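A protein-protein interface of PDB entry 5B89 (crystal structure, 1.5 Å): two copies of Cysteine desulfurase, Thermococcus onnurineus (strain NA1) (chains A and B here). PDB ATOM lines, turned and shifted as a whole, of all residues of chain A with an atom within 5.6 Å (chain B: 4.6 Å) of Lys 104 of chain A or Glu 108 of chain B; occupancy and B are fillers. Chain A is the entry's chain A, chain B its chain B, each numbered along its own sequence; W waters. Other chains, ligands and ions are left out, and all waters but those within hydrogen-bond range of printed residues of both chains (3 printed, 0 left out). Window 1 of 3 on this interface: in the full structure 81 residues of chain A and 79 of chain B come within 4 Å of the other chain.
Among the printed residues, merely in contact across the chains: Lys 104 of chain A with Leu 261 of chain B (3.9 Å), Leu 261 of chain A with Lys 104 of chain B (3.9 Å), Leu 261 of chain A with Asn 111 of chain B (3.4 Å) and Ala 286 of chain A with Ser 107 of chain B (3.8 Å).
The backbone carbonyl oxygen (O) of Ala 286 of chain A is in hydrogen-bond range of the side-chain amide nitrogen (ND2) of Asn 105 of chain B (3.1 Å).
The side-chain amino group of Lys 104 of chain A is in salt-bridge range of the side-chain carboxylate of Glu 108 of chain B (2.8 Å).
OE2 of Glu 108 of chain A is in salt-bridge range of NZ of Lys 104 of chain B (3.0 Å).
Of the 11 printed residues of chain B, 6 touch a printed residue of chain A.
Printed residues of chain B that touch a printed residue of chain A: Lys 104, Asn 105, Ser 107, Glu 108, Asn 111 and Leu 261.
Hydrophobic or aromatic side chains of chain B within 4 Å of the printed part of chain A: Leu 261.
Hydrophobic or aromatic side chains of chain A that line the printed part of chain B: Leu 261.
Along chain A the printed residues that touch a printed residue of chain B span positions 104 to 286.
Among the printed residues, 7 pairs touch across the chains.
Among the printed residues, Asp or Glu carboxylates within 4 Å of a Lys or Arg side-chain nitrogen of the other chain: Lys 104 of chain A with Glu 108 of chain B (2.8 Å) and Glu 108 of chain A with Lys 104 of chain B (3.0 Å).
N of Ile 244 of chain A is in hydrogen-bond range of O of Lys 104 of chain A, at 3.2 Å.
O of Asn 105 of chain B sits at hydrogen-bond distance from OG of Ser 109 of chain B (3.3 Å).
The side-chain amide oxygen (OD1) of Asn 105 of chain B lies within hydrogen-bond range of the backbone NH (N) of Glu 108 of chain B, at 2.7 Å.
The backbone NH (N) of Ser 107 of chain B is in hydrogen-bond range of the side-chain amide oxygen (OD1) of Asn 105 of chain B (3.2 Å).
The side-chain carboxylate of Glu 108 of chain A is in salt-bridge range of the side-chain amino group of Lys 104 of chain A, 2.9 Å away.
O of Ser 107 of chain B is in hydrogen-bond range of ND2 of Asn 111 of chain B (2.8 Å).
Water W3 lies within hydrogen-bond range of the side-chain amino group (NZ) of Lys 104 of chain B and the backbone carbonyl oxygen (O) of Ala 286 of chain A.
Water W1 bridges the side-chain carboxylate of Glu 108 of chain B (2.9 Å) and the side-chain amino group of Lys 104 of chain A (3.4 Å).
Water W2 lies within hydrogen-bond range of OE2 of Glu 108 of chain A, O of Phe 102 of chain A and NZ of Lys 104 of chain B.
Lys 104 of chain A touches two residues of chain B.
Of the printed residues of chain A, Asn 105 of chain B touches Ala 286 (3.1 Å).
Of the printed residues of chain A, Ser 107 of chain B touches Ala 286.
Lys 104 of chain A touches Glu 108 of chain B, and with the chains exchanged Glu 108 of chain A touches Lys 104 of chain B.
Lys 104 of chain A touches Leu 261 of chain B, and with the chains exchanged Leu 261 of chain A touches Lys 104 of chain B.
Of the 7 pairs that touch across the chains among the printed residues, 4 have their exchanged pair printed and touching as well.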
ATOM      1  N   PHE A 102     -16.928  21.689  19.631  1.00  0.00           N
ATOM      2  CA  PHE A 102     -16.587  21.949  18.219  1.00  0.00           C
ATOM      3  C   PHE A 102     -15.098  22.028  18.050  1.00  0.00           C
ATOM      4  O   PHE A 102     -14.339  22.671  18.834  1.00  0.00           O
ATOM      5  CB  PHE A 102     -17.304  23.171  17.715  1.00  0.00           C
ATOM      6  CG  PHE A 102     -18.796  22.964  17.593  1.00  0.00           C
ATOM      7  CD1 PHE A 102     -19.292  22.064  16.692  1.00  0.00           C
ATOM      8  CD2 PHE A 102     -19.699  23.793  18.249  1.00  0.00           C
ATOM      9  CE1 PHE A 102     -20.653  21.855  16.547  1.00  0.00           C
ATOM     10  CE2 PHE A 102     -21.048  23.601  17.993  1.00  0.00           C
ATOM     11  CZ  PHE A 102     -21.546  22.671  17.188  1.00  0.00           C
ATOM     12  N   THR A 103     -14.665  21.350  16.981  1.00  0.00           N
ATOM     13  CA  THR A 103     -13.266  21.268  16.564  1.00  0.00           C
ATOM     14  C   THR A 103     -13.224  21.566  15.048  1.00  0.00           C
ATOM     15  O   THR A 103     -14.202  21.869  14.479  1.00  0.00           O
ATOM     16  CB  THR A 103     -12.699  19.854  16.793  1.00  0.00           C
ATOM     17  OG1 THR A 103     -13.384  18.938  15.972  1.00  0.00           O
ATOM     18  CG2 THR A 103     -12.914  19.415  18.176  1.00  0.00           C
ATOM     19  N   LYS A 104     -12.052  21.477  14.426  1.00  0.00           N
ATOM     20  CA  LYS A 104     -11.977  21.726  12.972  1.00  0.00           C
ATOM     21  C   LYS A 104     -12.343  20.525  12.086  1.00  0.00           C
ATOM     22  O   LYS A 104     -12.751  20.669  11.020  1.00  0.00           O
ATOM     23  CB  LYS A 104     -10.621  22.364  12.579  1.00  0.00           C
ATOM     24  CG  LYS A 104      -9.610  21.404  12.082  1.00  0.00           C
ATOM     25  CD  LYS A 104      -8.363  22.050  11.459  1.00  0.00           C
ATOM     26  CE  LYS A 104      -7.587  22.789  12.523  1.00  0.00           C
ATOM     27  NZ  LYS A 104      -7.163  22.009  13.741  1.00  0.00           N
ATOM     28  N   ASN A 105     -12.144  19.340  12.633  1.00  0.00           N
ATOM     29  CA  ASN A 105     -12.392  18.101  11.941  1.00  0.00           C
ATOM     30  C   ASN A 105     -12.230  16.891  12.862  1.00  0.00           C
ATOM     31  O   ASN A 105     -11.888  17.071  13.975  1.00  0.00           O
ATOM     32  CB  ASN A 105     -11.471  18.019  10.724  1.00  0.00           C
ATOM     33  CG  ASN A 105      -9.998  18.083  11.075  1.00  0.00           C
ATOM     34  OD1 ASN A 105      -9.600  17.712  12.094  1.00  0.00           O
ATOM     35  ND2 ASN A 105      -9.220  18.587  10.182  1.00  0.00           N
ATOM     36  N   THR A 106     -12.525  15.680  12.349  1.00  0.00           N
ATOM     37  CA  THR A 106     -12.368  14.467  13.103  1.00  0.00           C
ATOM     38  C   THR A 106     -10.986  14.246  13.581  1.00  0.00           C
ATOM     39  O   THR A 106     -10.734  13.857  14.695  1.00  0.00           O
ATOM     40  CB  THR A 106     -12.744  13.266  12.306  1.00  0.00           C
ATOM     41  OG1 THR A 106     -14.192  13.309  12.010  1.00  0.00           O
ATOM     42  CG2 THR A 106     -12.495  11.998  12.954  1.00  0.00           C
ATOM     43  N   GLU A 108      -8.622  16.466  14.372  1.00  0.00           N
ATOM     44  CA  GLU A 108      -8.402  17.261  15.554  1.00  0.00           C
ATOM     45  C   GLU A 108      -9.058  16.596  16.803  1.00  0.00           C
ATOM     46  O   GLU A 108      -8.468  16.492  17.858  1.00  0.00           O
ATOM     47  CB  GLU A 108      -8.890  18.711  15.398  1.00  0.00           C
ATOM     48  CG  GLU A 108      -8.673  19.566  16.635  1.00  0.00           C
ATOM     49  CD  GLU A 108      -9.272  20.983  16.571  1.00  0.00           C
ATOM     50  OE1 GLU A 108      -9.416  21.546  15.501  1.00  0.00           O
ATOM     51  OE2 GLU A 108      -9.492  21.599  17.646  1.00  0.00           O
ATOM     52  N   THR A 242     -16.754  22.823   5.453  1.00  0.00           N
ATOM     53  CA  THR A 242     -15.479  22.430   5.906  1.00  0.00           C
ATOM     54  C   THR A 242     -15.137  23.220   7.182  1.00  0.00           C
ATOM     55  O   THR A 242     -15.768  24.171   7.504  1.00  0.00           O
ATOM     56  CB  THR A 242     -14.374  22.666   4.853  1.00  0.00           C
ATOM     57  OG1 THR A 242     -14.301  24.038   4.511  1.00  0.00           O
ATOM     58  CG2 THR A 242     -14.639  21.852   3.590  1.00  0.00           C
ATOM     59  N   GLY A 243     -14.123  22.774   7.895  1.00  0.00           N
ATOM     60  CA  GLY A 243     -13.663  23.468   9.074  1.00  0.00           C
ATOM     61  C   GLY A 243     -14.477  23.303  10.340  1.00  0.00           C
ATOM     62  O   GLY A 243     -14.301  24.028  11.229  1.00  0.00           O
ATOM     63  N   ILE A 244     -15.367  22.315  10.349  1.00  0.00           N
ATOM     64  CA  ILE A 244     -16.181  22.078  11.530  1.00  0.00           C
ATOM     65  C   ILE A 244     -16.266  20.584  11.806  1.00  0.00           C
ATOM     66  O   ILE A 244     -16.675  19.819  11.012  1.00  0.00           O
ATOM     67  CB  ILE A 244     -17.583  22.738  11.448  1.00  0.00           C
ATOM     68  CG1 ILE A 244     -18.334  22.677  12.786  1.00  0.00           C
ATOM     69  CG2 ILE A 244     -18.432  22.178  10.347  1.00  0.00           C
ATOM     70  CD1 ILE A 244     -17.724  23.621  13.793  1.00  0.00           C
ATOM     71  N   GLY A 245     -15.789  20.264  12.965  1.00  0.00           N
ATOM     72  CA  GLY A 245     -15.787  18.909  13.460  1.00  0.00           C
ATOM     73  C   GLY A 245     -16.447  18.874  14.811  1.00  0.00           C
ATOM     74  O   GLY A 245     -16.664  19.849  15.372  1.00  0.00           O
ATOM     75  N   LEU A 261      -6.291  22.578  24.516  1.00  0.00           N
ATOM     76  CA  LEU A 261      -6.242  23.947  24.038  1.00  0.00           C
ATOM     77  C   LEU A 261      -6.962  24.829  24.999  1.00  0.00           C
ATOM     78  O   LEU A 261      -8.149  24.573  25.257  1.00  0.00           O
ATOM     79  CB  LEU A 261      -6.937  24.046  22.632  1.00  0.00           C
ATOM     80  CG  LEU A 261      -6.422  23.030  21.608  1.00  0.00           C
ATOM     81  CD1 LEU A 261      -7.249  23.260  20.298  1.00  0.00           C
ATOM     82  CD2 LEU A 261      -4.903  23.030  21.339  1.00  0.00           C
ATOM     83  N   ALA A 286     -11.238  26.751  22.869  1.00  0.00           N
ATOM     84  CA  ALA A 286     -10.378  27.900  22.987  1.00  0.00           C
ATOM     85  C   ALA A 286     -10.460  28.839  21.782  1.00  0.00           C
ATOM     86  O   ALA A 286     -10.349  28.406  20.683  1.00  0.00           O
ATOM     87  CB  ALA A 286      -8.949  27.464  23.228  1.00  0.00           C
ATOM     88  N   THR B 103      -4.970  26.977  10.940  1.00  0.00           N
ATOM     89  CA  THR B 103      -5.559  26.564  12.199  1.00  0.00           C
ATOM     90  C   THR B 103      -6.999  27.075  12.272  1.00  0.00           C
ATOM     91  O   THR B 103      -7.491  27.575  11.332  1.00  0.00           O
ATOM     92  CB  THR B 103      -4.783  27.170  13.392  1.00  0.00           C
ATOM     93  OG1 THR B 103      -4.914  28.575  13.355  1.00  0.00           O
ATOM     94  CG2 THR B 103      -3.324  26.818  13.281  1.00  0.00           C
ATOM     95  N   LYS B 104      -7.636  26.939  13.427  1.00  0.00           N
ATOM     96  CA  LYS B 104      -9.011  27.441  13.533  1.00  0.00           C
ATOM     97  C   LYS B 104      -9.119  28.889  13.969  1.00  0.00           C
ATOM     98  O   LYS B 104     -10.063  29.528  13.713  1.00  0.00           O
ATOM     99  CB  LYS B 104      -9.921  26.545  14.405  1.00  0.00           C
ATOM    100  CG  LYS B 104      -9.963  26.881  15.843  1.00  0.00           C
ATOM    101  CD  LYS B 104     -11.112  26.167  16.552  1.00  0.00           C
ATOM    102  CE  LYS B 104     -10.719  24.718  16.660  1.00  0.00           C
ATOM    103  NZ  LYS B 104      -9.395  24.552  17.366  1.00  0.00           N
ATOM    104  N   ASN B 105      -8.093  29.355  14.642  1.00  0.00           N
ATOM    105  CA  ASN B 105      -8.043  30.708  15.183  1.00  0.00           C
ATOM    106  C   ASN B 105      -6.677  30.982  15.824  1.00  0.00           C
ATOM    107  O   ASN B 105      -5.874  30.129  15.894  1.00  0.00           O
ATOM    108  CB  ASN B 105      -9.172  30.949  16.221  1.00  0.00           C
ATOM    109  CG  ASN B 105      -9.170  29.943  17.365  1.00  0.00           C
ATOM    110  OD1 ASN B 105      -8.191  29.447  17.759  1.00  0.00           O
ATOM    111  ND2 ASN B 105     -10.345  29.652  17.844  1.00  0.00           N
ATOM    112  N   THR B 106      -6.501  32.199  16.285  1.00  0.00           N
ATOM    113  CA  THR B 106      -5.213  32.585  16.943  1.00  0.00           C
ATOM    114  C   THR B 106      -4.962  31.748  18.132  1.00  0.00           C
ATOM    115  O   THR B 106      -3.847  31.335  18.424  1.00  0.00           O
ATOM    116  CB  THR B 106      -5.211  34.056  17.329  1.00  0.00           C
ATOM    117  OG1 THR B 106      -5.257  34.893  16.169  1.00  0.00           O
ATOM    118  CG2 THR B 106      -4.054  34.442  18.142  1.00  0.00           C
ATOM    119  N   SER B 107      -6.027  31.477  18.904  1.00  0.00           N
ATOM    120  CA  SER B 107      -5.905  30.725  20.160  1.00  0.00           C
ATOM    121  C   SER B 107      -5.331  29.310  19.863  1.00  0.00           C
ATOM    122  O   SER B 107      -4.345  28.890  20.590  1.00  0.00           O
ATOM    123  CB  SER B 107      -7.222  30.583  20.846  1.00  0.00           C
ATOM    124  OG  SER B 107      -7.728  31.900  21.165  1.00  0.00           O
ATOM    125  N   GLU B 108      -5.846  28.606  18.867  1.00  0.00           N
ATOM    126  CA  GLU B 108      -5.288  27.312  18.453  1.00  0.00           C
ATOM    127  C   GLU B 108      -3.799  27.521  18.085  1.00  0.00           C
ATOM    128  O   GLU B 108      -2.928  26.780  18.570  1.00  0.00           O
ATOM    129  CB  GLU B 108      -6.045  26.640  17.333  1.00  0.00           C
ATOM    130  CG  GLU B 108      -5.449  25.305  16.925  1.00  0.00           C
ATOM    131  CD  GLU B 108      -6.099  24.707  15.657  1.00  0.00           C
ATOM    132  OE1 GLU B 108      -7.279  24.947  15.418  1.00  0.00           O
ATOM    133  OE2 GLU B 108      -5.467  23.826  15.043  1.00  0.00           O
ATOM    134  N   SER B 109      -3.501  28.525  17.234  1.00  0.00           N
ATOM    135  CA  SER B 109      -2.122  28.742  16.839  1.00  0.00           C
ATOM    136  C   SER B 109      -1.158  28.924  18.008  1.00  0.00           C
ATOM    137  O   SER B 109      -0.089  28.243  18.048  1.00  0.00           O
ATOM    138  CB  SER B 109      -2.036  29.985  15.997  1.00  0.00           C
ATOM    139  OG  SER B 109      -2.751  29.862  14.778  1.00  0.00           O
ATOM    140  N   LEU B 110      -1.536  29.711  19.011  1.00  0.00           N
ATOM    141  CA  LEU B 110      -0.621  29.930  20.150  1.00  0.00           C
ATOM    142  C   LEU B 110      -0.498  28.704  21.038  1.00  0.00           C
ATOM    143  O   LEU B 110       0.595  28.376  21.471  1.00  0.00           O
ATOM    144  CB  LEU B 110      -1.104  31.124  20.993  1.00  0.00           C
ATOM    145  CG  LEU B 110      -1.028  32.470  20.272  1.00  0.00           C
ATOM    146  CD1 LEU B 110      -1.812  33.559  21.002  1.00  0.00           C
ATOM    147  CD2 LEU B 110       0.401  32.962  20.000  1.00  0.00           C
ATOM    148  N   ASN B 111      -1.576  27.972  21.202  1.00  0.00           N
ATOM    149  CA  ASN B 111      -1.502  26.692  21.936  1.00  0.00           C
ATOM    150  C   ASN B 111      -0.577  25.746  21.187  1.00  0.00           C
ATOM    151  O   ASN B 111       0.186  25.022  21.812  1.00  0.00           O
ATOM    152  CB  ASN B 111      -2.870  26.035  22.075  1.00  0.00           C
ATOM    153  CG  ASN B 111      -3.610  26.541  23.301  1.00  0.00           C
ATOM    154  OD1 ASN B 111      -3.551  25.951  24.407  1.00  0.00           O
ATOM    155  ND2 ASN B 111      -4.367  27.627  23.144  1.00  0.00           N
ATOM    156  N   LEU B 112      -0.665  25.683  19.843  1.00  0.00           N
ATOM    157  CA  LEU B 112       0.227  24.797  19.065  1.00  0.00           C
ATOM    158  C   LEU B 112       1.672  25.170  19.262  1.00  0.00           C
ATOM    159  O   LEU B 112       2.523  24.255  19.298  1.00  0.00           O
ATOM    160  CB  LEU B 112      -0.146  24.783  17.590  1.00  0.00           C
ATOM    161  CG  LEU B 112      -1.503  24.191  17.253  1.00  0.00           C
ATOM    162  CD1 LEU B 112      -1.645  24.355  15.742  1.00  0.00           C
ATOM    163  CD2 LEU B 112      -1.639  22.770  17.732  1.00  0.00           C
ATOM    164  N   LEU B 261      -0.638  18.089  16.375  1.00  0.00           N
ATOM    165  CA  LEU B 261      -1.782  17.387  15.781  1.00  0.00           C
ATOM    166  C   LEU B 261      -1.287  16.608  14.571  1.00  0.00           C
ATOM    167  O   LEU B 261      -0.734  17.172  13.584  1.00  0.00           O
ATOM    168  CB  LEU B 261      -2.902  18.331  15.353  1.00  0.00           C
ATOM    169  CG  LEU B 261      -3.378  19.312  16.414  1.00  0.00           C
ATOM    170  CD1 LEU B 261      -4.366  20.293  15.839  1.00  0.00           C
ATOM    171  CD2 LEU B 261      -3.928  18.637  17.625  1.00  0.00           C
HETATM  172  O   HOH W   1      -4.156  23.145  12.587  1.00  0.00           O
HETATM  173  O   HOH W   2     -11.466  22.785  19.363  1.00  0.00           O
HETATM  174  O   HOH W   3      -9.006  26.159  19.620  1.00  0.00           O
